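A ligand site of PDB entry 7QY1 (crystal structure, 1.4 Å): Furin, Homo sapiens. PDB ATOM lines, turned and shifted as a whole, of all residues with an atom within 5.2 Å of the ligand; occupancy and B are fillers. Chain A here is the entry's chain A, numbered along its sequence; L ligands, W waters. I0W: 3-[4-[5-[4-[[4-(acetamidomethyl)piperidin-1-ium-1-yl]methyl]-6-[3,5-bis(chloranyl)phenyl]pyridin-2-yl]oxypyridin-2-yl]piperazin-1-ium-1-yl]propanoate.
O of Leu 45 touches CL2 of the ligand, at 3.1 Å. His 87 touches the ligand (CD2 to OBP, 3.7 Å). Met 119 touches the ligand. Leu 120 touches the ligand (CD2 to CAZ, 3.7 Å). O of Val 124 touches CAK of the ligand, at 3.4 Å. CB of Asp 126 touches OAC of the ligand, at 3.7 Å. Leu 133 touches the ligand (CG to CL1, 3.6 Å). Ala 145 touches the ligand. Trp 147 touches the ligand. Gly 148 touches the ligand (O to CBG, 3.4 Å). N of Pro 149 touches CAM of the ligand (3.9 Å). Asp 157 touches the ligand. Gly 158 touches the ligand (O to CAH, 3.5 Å). Ala 160 touches the ligand. Trp 184 touches the ligand. Hydrophobic or aromatic side chains within 4 Å of the ligand: His 87, Met 119, Leu 120, Val 124, Leu 133, Ala 145, Trp 147, Ala 160, Trp 184 and Tyr 201. Along chain A the residues within 4 Å of the ligand span positions 45 to 201.
The side-chain carboxylate (OE1) of Glu 129 is in hydrogen-bond range of the side-chain hydroxyl (OH) of Tyr 201 (2.5 Å). The indole nitrogen of Trp 147 lies within hydrogen-bond range of a ring nitrogen (ND1) of His 87 (3.5 Å). NE1 of Trp 184 lies within hydrogen-bond range of O of Trp 147, 2.9 Å away. NE1 of Trp 147 sits at hydrogen-bond distance from OD2 of Asp 46, at 3.0 Å. The backbone NH of Met 119 is in hydrogen-bond range of the backbone carbonyl oxygen of Asp 46. OD2 of Asp 46 lies within hydrogen-bond range of ND1 of His 87 (2.8 Å). The side-chain carboxylate (OD2) of Asp 47 is in hydrogen-bond range of the backbone NH (N) of His 87, 3.0 Å away. The backbone NH (N) of Leu 120 sits at hydrogen-bond distance from the backbone carbonyl oxygen (O) of Asp 46, 3.1 Å away.
Water W8 lies within hydrogen-bond range of OBP of the ligand (2.7 Å) and NE of Arg 86 (2.9 Å). Water W7 bridges an oxygen (OAC) of the ligand (2.7 Å) and the backbone NH (N) of Asp 126 (2.9 Å). Water W2 lies within hydrogen-bond range of OD1 of Asp 46, NBK of the ligand and OD2 of Asp 47. Water W1 bridges OD2 of Asp 157 (2.8 Å) and NAD of the ligand (2.9 Å). Water W4 bridges OD2 of Asp 47 and N of Asn 85.
The side-chain carboxylate (OE2) of Glu 129 is in salt-bridge range of a nitrogen (NAI) of the ligand, at 2.7 Å. NAI of the ligand is in hydrogen-bond range of OH of Tyr 201 (3.1 Å).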
ATOM      1  N   LEU A  45      -3.996  -4.377 -11.229  1.00  0.00           N
ATOM      2  CA  LEU A  45      -3.259  -5.619 -11.432  1.00  0.00           C
ATOM      3  C   LEU A  45      -1.798  -5.233 -11.684  1.00  0.00           C
ATOM      4  O   LEU A  45      -1.432  -4.779 -12.764  1.00  0.00           O
ATOM      5  CB  LEU A  45      -3.854  -6.408 -12.592  1.00  0.00           C
ATOM      6  CG  LEU A  45      -5.020  -7.335 -12.234  1.00  0.00           C
ATOM      7  CD1 LEU A  45      -6.130  -6.576 -11.583  1.00  0.00           C
ATOM      8  CD2 LEU A  45      -5.549  -8.048 -13.478  1.00  0.00           C
ATOM      9  N   ASP A  46      -0.944  -5.406 -10.670  1.00  0.00           N
ATOM     10  CA  ASP A  46       0.428  -4.908 -10.765  1.00  0.00           C
ATOM     11  C   ASP A  46       1.329  -5.558  -9.705  1.00  0.00           C
ATOM     12  O   ASP A  46       1.201  -6.754  -9.447  1.00  0.00           O
ATOM     13  CB  ASP A  46       0.357  -3.372 -10.632  1.00  0.00           C
ATOM     14  CG  ASP A  46       1.448  -2.649 -11.416  1.00  0.00           C
ATOM     15  OD1 ASP A  46       2.619  -2.896 -11.152  1.00  0.00           O
ATOM     16  OD2 ASP A  46       1.130  -1.799 -12.258  1.00  0.00           O
ATOM     17  N   ASP A  47       2.243  -4.780  -9.128  1.00  0.00           N
ATOM     18  CA  ASP A  47       3.274  -5.297  -8.235  1.00  0.00           C
ATOM     19  C   ASP A  47       2.922  -5.144  -6.758  1.00  0.00           C
ATOM     20  O   ASP A  47       3.788  -5.365  -5.902  1.00  0.00           O
ATOM     21  CB  ASP A  47       4.615  -4.627  -8.519  1.00  0.00           C
ATOM     22  CG  ASP A  47       4.541  -3.117  -8.451  1.00  0.00           C
ATOM     23  OD1 ASP A  47       3.576  -2.595  -7.844  1.00  0.00           O
ATOM     24  OD2 ASP A  47       5.446  -2.446  -9.027  1.00  0.00           O
ATOM     25  N   ASN A  85       8.609  -2.299  -6.870  1.00  0.00           N
ATOM     26  CA  ASN A  85       7.271  -2.631  -6.420  1.00  0.00           C
ATOM     27  C   ASN A  85       6.510  -1.419  -5.985  1.00  0.00           C
ATOM     28  O   ASN A  85       5.621  -1.533  -5.121  1.00  0.00           O
ATOM     29  CB  ASN A  85       7.327  -3.715  -5.348  1.00  0.00           C
ATOM     30  CG  ASN A  85       8.011  -4.959  -5.847  1.00  0.00           C
ATOM     31  OD1 ASN A  85       7.692  -5.466  -6.917  1.00  0.00           O
ATOM     32  ND2 ASN A  85       9.014  -5.418  -5.113  1.00  0.00           N
ATOM     33  N   ARG A  86       6.765  -0.278  -6.617  1.00  0.00           N
ATOM     34  CA  ARG A  86       6.002   0.929  -6.317  1.00  0.00           C
ATOM     35  C   ARG A  86       4.899   1.203  -7.318  1.00  0.00           C
ATOM     36  O   ARG A  86       4.090   2.092  -7.081  1.00  0.00           O
ATOM     37  CB  ARG A  86       6.926   2.148  -6.250  1.00  0.00           C
ATOM     38  CG  ARG A  86       7.525   2.500  -7.554  1.00  0.00           C
ATOM     39  CD  ARG A  86       8.645   3.509  -7.362  1.00  0.00           C
ATOM     40  NE  ARG A  86       9.110   3.882  -8.669  1.00  0.00           N
ATOM     41  CZ  ARG A  86      10.088   4.732  -8.912  1.00  0.00           C
ATOM     42  NH1 ARG A  86      10.734   5.327  -7.911  1.00  0.00           N
ATOM     43  NH2 ARG A  86      10.391   4.975 -10.170  1.00  0.00           N
ATOM     44  N   HIS A  87       4.868   0.479  -8.436  1.00  0.00           N
ATOM     45  CA  HIS A  87       4.040   0.934  -9.544  1.00  0.00           C
ATOM     46  C   HIS A  87       2.560   0.770  -9.245  1.00  0.00           C
ATOM     47  O   HIS A  87       1.759   1.653  -9.568  1.00  0.00           O
ATOM     48  CB  HIS A  87       4.414   0.227 -10.850  1.00  0.00           C
ATOM     49  CG  HIS A  87       3.849   0.891 -12.061  1.00  0.00           C
ATOM     50  ND1 HIS A  87       2.659   0.506 -12.632  1.00  0.00           N
ATOM     51  CD2 HIS A  87       4.294   1.949 -12.788  1.00  0.00           C
ATOM     52  CE1 HIS A  87       2.391   1.293 -13.662  1.00  0.00           C
ATOM     53  NE2 HIS A  87       3.365   2.174 -13.784  1.00  0.00           N
ATOM     54  N   MET A 119       0.668  -9.388  -8.446  1.00  0.00           N
ATOM     55  CA  MET A 119       0.858 -10.474  -9.397  1.00  0.00           C
ATOM     56  C   MET A 119       2.157 -10.402 -10.190  1.00  0.00           C
ATOM     57  O   MET A 119       2.569 -11.434 -10.734  1.00  0.00           O
ATOM     58  CB  MET A 119      -0.304 -10.535 -10.399  1.00  0.00           C
ATOM     59  CG  MET A 119      -0.406  -9.312 -11.278  1.00  0.00           C
ATOM     60  SD  MET A 119      -1.711  -9.388 -12.532  1.00  0.00           S
ATOM     61  CE  MET A 119      -1.089 -10.760 -13.502  1.00  0.00           C
ATOM     62  N   LEU A 120       2.811  -9.234 -10.288  1.00  0.00           N
ATOM     63  CA  LEU A 120       3.986  -9.071 -11.123  1.00  0.00           C
ATOM     64  C   LEU A 120       5.303  -9.262 -10.357  1.00  0.00           C
ATOM     65  O   LEU A 120       6.379  -9.176 -10.973  1.00  0.00           O
ATOM     66  CB  LEU A 120       3.995  -7.704 -11.815  1.00  0.00           C
ATOM     67  CG  LEU A 120       2.769  -7.421 -12.706  1.00  0.00           C
ATOM     68  CD1 LEU A 120       2.887  -6.041 -13.387  1.00  0.00           C
ATOM     69  CD2 LEU A 120       2.572  -8.525 -13.774  1.00  0.00           C
ATOM     70  N   VAL A 124       5.153 -14.836 -13.752  1.00  0.00           N
ATOM     71  CA  VAL A 124       3.794 -14.610 -14.232  1.00  0.00           C
ATOM     72  C   VAL A 124       3.457 -15.769 -15.177  1.00  0.00           C
ATOM     73  O   VAL A 124       3.924 -15.813 -16.319  1.00  0.00           O
ATOM     74  CB  VAL A 124       3.642 -13.265 -14.934  1.00  0.00           C
ATOM     75  CG1 VAL A 124       2.237 -13.112 -15.444  1.00  0.00           C
ATOM     76  CG2 VAL A 124       4.018 -12.124 -13.977  1.00  0.00           C
ATOM     77  N   THR A 125       2.679 -16.708 -14.668  1.00  0.00           N
ATOM     78  CA  THR A 125       2.200 -17.841 -15.430  1.00  0.00           C
ATOM     79  C   THR A 125       0.758 -17.575 -15.863  1.00  0.00           C
ATOM     80  O   THR A 125       0.095 -16.654 -15.402  1.00  0.00           O
ATOM     81  CB  THR A 125       2.189 -19.082 -14.541  1.00  0.00           C
ATOM     82  OG1 THR A 125       1.297 -18.825 -13.460  1.00  0.00           O
ATOM     83  CG2 THR A 125       3.575 -19.443 -14.019  1.00  0.00           C
ATOM     84  N   ASP A 126       0.270 -18.432 -16.761  1.00  0.00           N
ATOM     85  CA  ASP A 126      -1.125 -18.380 -17.155  1.00  0.00           C
ATOM     86  C   ASP A 126      -2.053 -18.473 -15.956  1.00  0.00           C
ATOM     87  O   ASP A 126      -3.036 -17.727 -15.862  1.00  0.00           O
ATOM     88  CB  ASP A 126      -1.361 -19.516 -18.159  1.00  0.00           C
ATOM     89  CG  ASP A 126      -2.760 -19.554 -18.742  1.00  0.00           C
ATOM     90  OD1 ASP A 126      -3.357 -18.475 -19.019  1.00  0.00           O
ATOM     91  OD2 ASP A 126      -3.239 -20.687 -18.959  1.00  0.00           O
ATOM     92  N   GLU A 129      -2.122 -15.179 -14.074  1.00  0.00           N
ATOM     93  CA  GLU A 129      -2.944 -14.199 -14.781  1.00  0.00           C
ATOM     94  C   GLU A 129      -4.423 -14.498 -14.602  1.00  0.00           C
ATOM     95  O   GLU A 129      -5.219 -13.582 -14.364  1.00  0.00           O
ATOM     96  CB  GLU A 129      -2.589 -14.217 -16.266  1.00  0.00           C
ATOM     97  CG  GLU A 129      -1.148 -13.821 -16.552  1.00  0.00           C
ATOM     98  CD  GLU A 129      -0.805 -13.837 -18.029  1.00  0.00           C
ATOM     99  OE1 GLU A 129      -1.736 -13.946 -18.856  1.00  0.00           O
ATOM    100  OE2 GLU A 129       0.384 -13.785 -18.367  1.00  0.00           O
ATOM    101  N   LEU A 133      -7.181 -11.821 -13.101  1.00  0.00           N
ATOM    102  CA  LEU A 133      -8.290 -11.310 -13.878  1.00  0.00           C
ATOM    103  C   LEU A 133      -9.616 -11.783 -13.316  1.00  0.00           C
ATOM    104  O   LEU A 133     -10.624 -11.088 -13.436  1.00  0.00           O
ATOM    105  CB  LEU A 133      -8.168 -11.821 -15.302  1.00  0.00           C
ATOM    106  CG  LEU A 133      -6.985 -11.275 -16.119  1.00  0.00           C
ATOM    107  CD1 LEU A 133      -6.757 -12.185 -17.338  1.00  0.00           C
ATOM    108  CD2 LEU A 133      -7.218  -9.838 -16.488  1.00  0.00           C
ATOM    109  N   ALA A 145      -4.953  -2.781 -15.826  1.00  0.00           N
ATOM    110  CA  ALA A 145      -3.696  -3.463 -16.060  1.00  0.00           C
ATOM    111  C   ALA A 145      -2.836  -2.663 -17.010  1.00  0.00           C
ATOM    112  O   ALA A 145      -3.249  -2.353 -18.138  1.00  0.00           O
ATOM    113  CB  ALA A 145      -3.919  -4.866 -16.631  1.00  0.00           C
ATOM    114  N   SER A 146      -1.598  -2.388 -16.610  1.00  0.00           N
ATOM    115  CA  SER A 146      -0.728  -1.494 -17.350  1.00  0.00           C
ATOM    116  C   SER A 146       0.373  -2.193 -18.133  1.00  0.00           C
ATOM    117  O   SER A 146       1.199  -1.514 -18.741  1.00  0.00           O
ATOM    118  CB  SER A 146      -0.116  -0.453 -16.398  1.00  0.00           C
ATOM    119  OG  SER A 146      -1.101   0.485 -16.011  1.00  0.00           O
ATOM    120  N   TRP A 147       0.379  -3.531 -18.155  1.00  0.00           N
ATOM    121  CA  TRP A 147       1.523  -4.296 -18.644  1.00  0.00           C
ATOM    122  C   TRP A 147       1.039  -5.554 -19.363  1.00  0.00           C
ATOM    123  O   TRP A 147      -0.113  -5.969 -19.256  1.00  0.00           O
ATOM    124  CB  TRP A 147       2.438  -4.707 -17.488  1.00  0.00           C
ATOM    125  CG  TRP A 147       2.765  -3.588 -16.537  1.00  0.00           C
ATOM    126  CD1 TRP A 147       2.192  -3.356 -15.319  1.00  0.00           C
ATOM    127  CD2 TRP A 147       3.755  -2.555 -16.715  1.00  0.00           C
ATOM    128  NE1 TRP A 147       2.762  -2.259 -14.723  1.00  0.00           N
ATOM    129  CE2 TRP A 147       3.709  -1.740 -15.562  1.00  0.00           C
ATOM    130  CE3 TRP A 147       4.678  -2.236 -17.726  1.00  0.00           C
ATOM    131  CZ2 TRP A 147       4.550  -0.629 -15.392  1.00  0.00           C
ATOM    132  CZ3 TRP A 147       5.477  -1.124 -17.583  1.00  0.00           C
ATOM    133  CH2 TRP A 147       5.424  -0.331 -16.410  1.00  0.00           C
ATOM    134  N   GLY A 148       1.974  -6.203 -20.046  1.00  0.00           N
ATOM    135  CA  GLY A 148       1.680  -7.405 -20.796  1.00  0.00           C
ATOM    136  C   GLY A 148       2.954  -8.081 -21.243  1.00  0.00           C
ATOM    137  O   GLY A 148       3.983  -8.032 -20.556  1.00  0.00           O
ATOM    138  N   PRO A 149       2.909  -8.731 -22.399  1.00  0.00           N
ATOM    139  CA  PRO A 149       4.145  -9.308 -22.953  1.00  0.00           C
ATOM    140  C   PRO A 149       5.189  -8.228 -23.201  1.00  0.00           C
ATOM    141  O   PRO A 149       4.887  -7.043 -23.312  1.00  0.00           O
ATOM    142  CB  PRO A 149       3.689  -9.923 -24.286  1.00  0.00           C
ATOM    143  CG  PRO A 149       2.279  -9.874 -24.291  1.00  0.00           C
ATOM    144  CD  PRO A 149       1.785  -8.859 -23.327  1.00  0.00           C
ATOM    145  N   ASP A 157       2.548 -12.337 -28.363  1.00  0.00           N
ATOM    146  CA  ASP A 157       2.010 -13.212 -27.341  1.00  0.00           C
ATOM    147  C   ASP A 157       0.776 -12.578 -26.742  1.00  0.00           C
ATOM    148  O   ASP A 157       0.534 -11.373 -26.881  1.00  0.00           O
ATOM    149  CB  ASP A 157       3.045 -13.522 -26.239  1.00  0.00           C
ATOM    150  CG  ASP A 157       2.798 -14.876 -25.554  1.00  0.00           C
ATOM    151  OD1 ASP A 157       1.832 -15.608 -25.928  1.00  0.00           O
ATOM    152  OD2 ASP A 157       3.597 -15.200 -24.651  1.00  0.00           O
ATOM    153  N   GLY A 158      -0.014 -13.411 -26.085  1.00  0.00           N
ATOM    154  CA  GLY A 158      -1.270 -13.000 -25.532  1.00  0.00           C
ATOM    155  C   GLY A 158      -1.687 -13.984 -24.455  1.00  0.00           C
ATOM    156  O   GLY A 158      -0.928 -14.886 -24.089  1.00  0.00           O
ATOM    157  N   PRO A 159      -2.898 -13.812 -23.942  1.00  0.00           N
ATOM    158  CA  PRO A 159      -3.375 -14.726 -22.896  1.00  0.00           C
ATOM    159  C   PRO A 159      -3.406 -16.167 -23.382  1.00  0.00           C
ATOM    160  O   PRO A 159      -3.917 -16.469 -24.465  1.00  0.00           O
ATOM    161  CB  PRO A 159      -4.781 -14.207 -22.573  1.00  0.00           C
ATOM    162  CG  PRO A 159      -5.202 -13.406 -23.797  1.00  0.00           C
ATOM    163  CD  PRO A 159      -3.913 -12.801 -24.309  1.00  0.00           C
ATOM    164  N   ALA A 160      -2.835 -17.055 -22.571  1.00  0.00           N
ATOM    165  CA  ALA A 160      -2.937 -18.492 -22.758  1.00  0.00           C
ATOM    166  C   ALA A 160      -4.319 -18.930 -22.277  1.00  0.00           C
ATOM    167  O   ALA A 160      -5.211 -18.098 -22.054  1.00  0.00           O
ATOM    168  CB  ALA A 160      -1.741 -19.192 -22.112  1.00  0.00           C
ATOM    169  N   TRP A 184      -6.854  -1.606 -20.224  1.00  0.00           N
ATOM    170  CA  TRP A 184      -5.501  -2.007 -20.546  1.00  0.00           C
ATOM    171  C   TRP A 184      -4.702  -0.851 -21.130  1.00  0.00           C
ATOM    172  O   TRP A 184      -5.237  -0.019 -21.860  1.00  0.00           O
ATOM    173  CB  TRP A 184      -5.432  -3.171 -21.553  1.00  0.00           C
ATOM    174  CG  TRP A 184      -4.475  -4.235 -21.109  1.00  0.00           C
ATOM    175  CD1 TRP A 184      -3.130  -4.315 -21.388  1.00  0.00           C
ATOM    176  CD2 TRP A 184      -4.769  -5.333 -20.254  1.00  0.00           C
ATOM    177  NE1 TRP A 184      -2.588  -5.406 -20.755  1.00  0.00           N
ATOM    178  CE2 TRP A 184      -3.567  -6.049 -20.049  1.00  0.00           C
ATOM    179  CE3 TRP A 184      -5.938  -5.791 -19.646  1.00  0.00           C
ATOM    180  CZ2 TRP A 184      -3.509  -7.207 -19.292  1.00  0.00           C
ATOM    181  CZ3 TRP A 184      -5.865  -6.934 -18.868  1.00  0.00           C
ATOM    182  CH2 TRP A 184      -4.667  -7.637 -18.711  1.00  0.00           C
ATOM    183  N   TYR A 201      -3.312  -9.030 -25.080  1.00  0.00           N
ATOM    184  CA  TYR A 201      -4.139  -8.472 -24.023  1.00  0.00           C
ATOM    185  C   TYR A 201      -4.789  -7.172 -24.493  1.00  0.00           C
ATOM    186  O   TYR A 201      -6.009  -7.031 -24.456  1.00  0.00           O
ATOM    187  CB  TYR A 201      -3.302  -8.251 -22.741  1.00  0.00           C
ATOM    188  CG  TYR A 201      -2.669  -9.525 -22.248  1.00  0.00           C
ATOM    189  CD1 TYR A 201      -1.524 -10.005 -22.844  1.00  0.00           C
ATOM    190  CD2 TYR A 201      -3.233 -10.268 -21.226  1.00  0.00           C
ATOM    191  CE1 TYR A 201      -0.941 -11.180 -22.451  1.00  0.00           C
ATOM    192  CE2 TYR A 201      -2.645 -11.468 -20.806  1.00  0.00           C
ATOM    193  CZ  TYR A 201      -1.513 -11.915 -21.442  1.00  0.00           C
ATOM    194  OH  TYR A 201      -0.909 -13.080 -21.070  1.00  0.00           O
HETATM  195  CAA I0W L   1       1.538 -21.021 -22.887  1.00  0.00           C
HETATM  196  CAB I0W L   1       1.575 -20.279 -21.549  1.00  0.00           C
HETATM  197  CAE I0W L   1       2.119 -18.226 -20.383  1.00  0.00           C
HETATM  198  CAF I0W L   1       2.469 -16.791 -20.735  1.00  0.00           C
HETATM  199  CAG I0W L   1       1.328 -16.111 -21.504  1.00  0.00           C
HETATM  200  CAH I0W L   1       1.730 -14.669 -21.800  1.00  0.00           C
HETATM  201  CAJ I0W L   1       3.070 -14.533 -19.773  1.00  0.00           C
HETATM  202  CAK I0W L   1       2.707 -15.995 -19.436  1.00  0.00           C
HETATM  203  CAL I0W L   1       2.399 -12.503 -20.965  1.00  0.00           C
HETATM  204  CAM I0W L   1       2.477 -11.563 -19.746  1.00  0.00           C
HETATM  205  CAN I0W L   1       3.708 -11.266 -19.174  1.00  0.00           C
HETATM  206  CAO I0W L   1       3.768 -10.423 -18.073  1.00  0.00           C
HETATM  207  CAQ I0W L   1       1.471 -10.110 -18.109  1.00  0.00           C
HETATM  208  CAR I0W L   1       1.346 -10.948 -19.208  1.00  0.00           C
HETATM  209  CAS I0W L   1       0.347  -9.522 -17.501  1.00  0.00           C
HETATM  210  CAT I0W L   1      -0.859 -10.218 -17.477  1.00  0.00           C
HETATM  211  CAU I0W L   1      -1.973  -9.681 -16.816  1.00  0.00           C
HETATM  212  CAW I0W L   1      -1.898  -8.451 -16.192  1.00  0.00           C
HETATM  213  CAX I0W L   1      -0.694  -7.774 -16.189  1.00  0.00           C
HETATM  214  CAZ I0W L   1       0.413  -8.305 -16.821  1.00  0.00           C
HETATM  215  CBB I0W L   1       5.303  -9.078 -16.850  1.00  0.00           C
HETATM  216  CBC I0W L   1       6.044  -9.223 -15.689  1.00  0.00           C
HETATM  217  CBD I0W L   1       6.462  -8.089 -14.996  1.00  0.00           C
HETATM  218  CBE I0W L   1       6.149  -6.828 -15.485  1.00  0.00           C
HETATM  219  CBG I0W L   1       4.990  -7.817 -17.325  1.00  0.00           C
HETATM  220  CBI I0W L   1       7.240  -5.816 -13.528  1.00  0.00           C
HETATM  221  CBJ I0W L   1       8.134  -4.601 -13.256  1.00  0.00           C
HETATM  222  CBL I0W L   1       8.373  -2.156 -13.209  1.00  0.00           C
HETATM  223  CBM I0W L   1       7.593  -0.764 -13.465  1.00  0.00           C
HETATM  224  CBN I0W L   1       8.213   0.230 -12.557  1.00  0.00           C
HETATM  225  CBQ I0W L   1       7.127  -3.288 -14.961  1.00  0.00           C
HETATM  226  CBR I0W L   1       6.152  -4.394 -15.290  1.00  0.00           C
HETATM  227  NAD I0W L   1       2.034 -19.042 -21.610  1.00  0.00           N
HETATM  228  NAI I0W L   1       2.009 -13.882 -20.567  1.00  0.00           N
HETATM  229  NAP I0W L   1       2.681  -9.860 -17.574  1.00  0.00           N
HETATM  230  NBF I0W L   1       5.412  -6.697 -16.597  1.00  0.00           N
HETATM  231  NBH I0W L   1       6.542  -5.719 -14.813  1.00  0.00           N
HETATM  232  NBK I0W L   1       7.491  -3.312 -13.528  1.00  0.00           N
HETATM  233  OAC I0W L   1       1.196 -20.827 -20.523  1.00  0.00           O
HETATM  234  OBA I0W L   1       4.989 -10.204 -17.539  1.00  0.00           O
HETATM  235  OBO I0W L   1       8.858  -0.133 -11.546  1.00  0.00           O
HETATM  236  OBP I0W L   1       7.956   1.405 -12.861  1.00  0.00           O
HETATM  237 CL1  I0W L   1      -3.468 -10.550 -16.763  1.00  0.00          CL
HETATM  238 CL2  I0W L   1      -0.587  -6.236 -15.374  1.00  0.00          CL
HETATM  239  O   HOH W   1       3.403 -17.890 -23.954  1.00  0.00           O
HETATM  240  O   HOH W   2       5.297  -3.042 -11.849  1.00  0.00           O
HETATM  241  O   HOH W   3       4.942 -13.494 -23.002  1.00  0.00           O
HETATM  242  O   HOH W   4       7.829  -3.439 -10.039  1.00  0.00           O
HETATM  243  O   HOH W   5       6.668  -8.424 -20.075  1.00  0.00           O
HETATM  244  O   HOH W   6       7.398   2.680 -15.099  1.00  0.00           O
HETATM  245  O   HOH W   7       1.994 -20.506 -17.925  1.00  0.00           O
HETATM  246  O   HOH W   8       7.524   3.233 -10.947  1.00  0.00           O
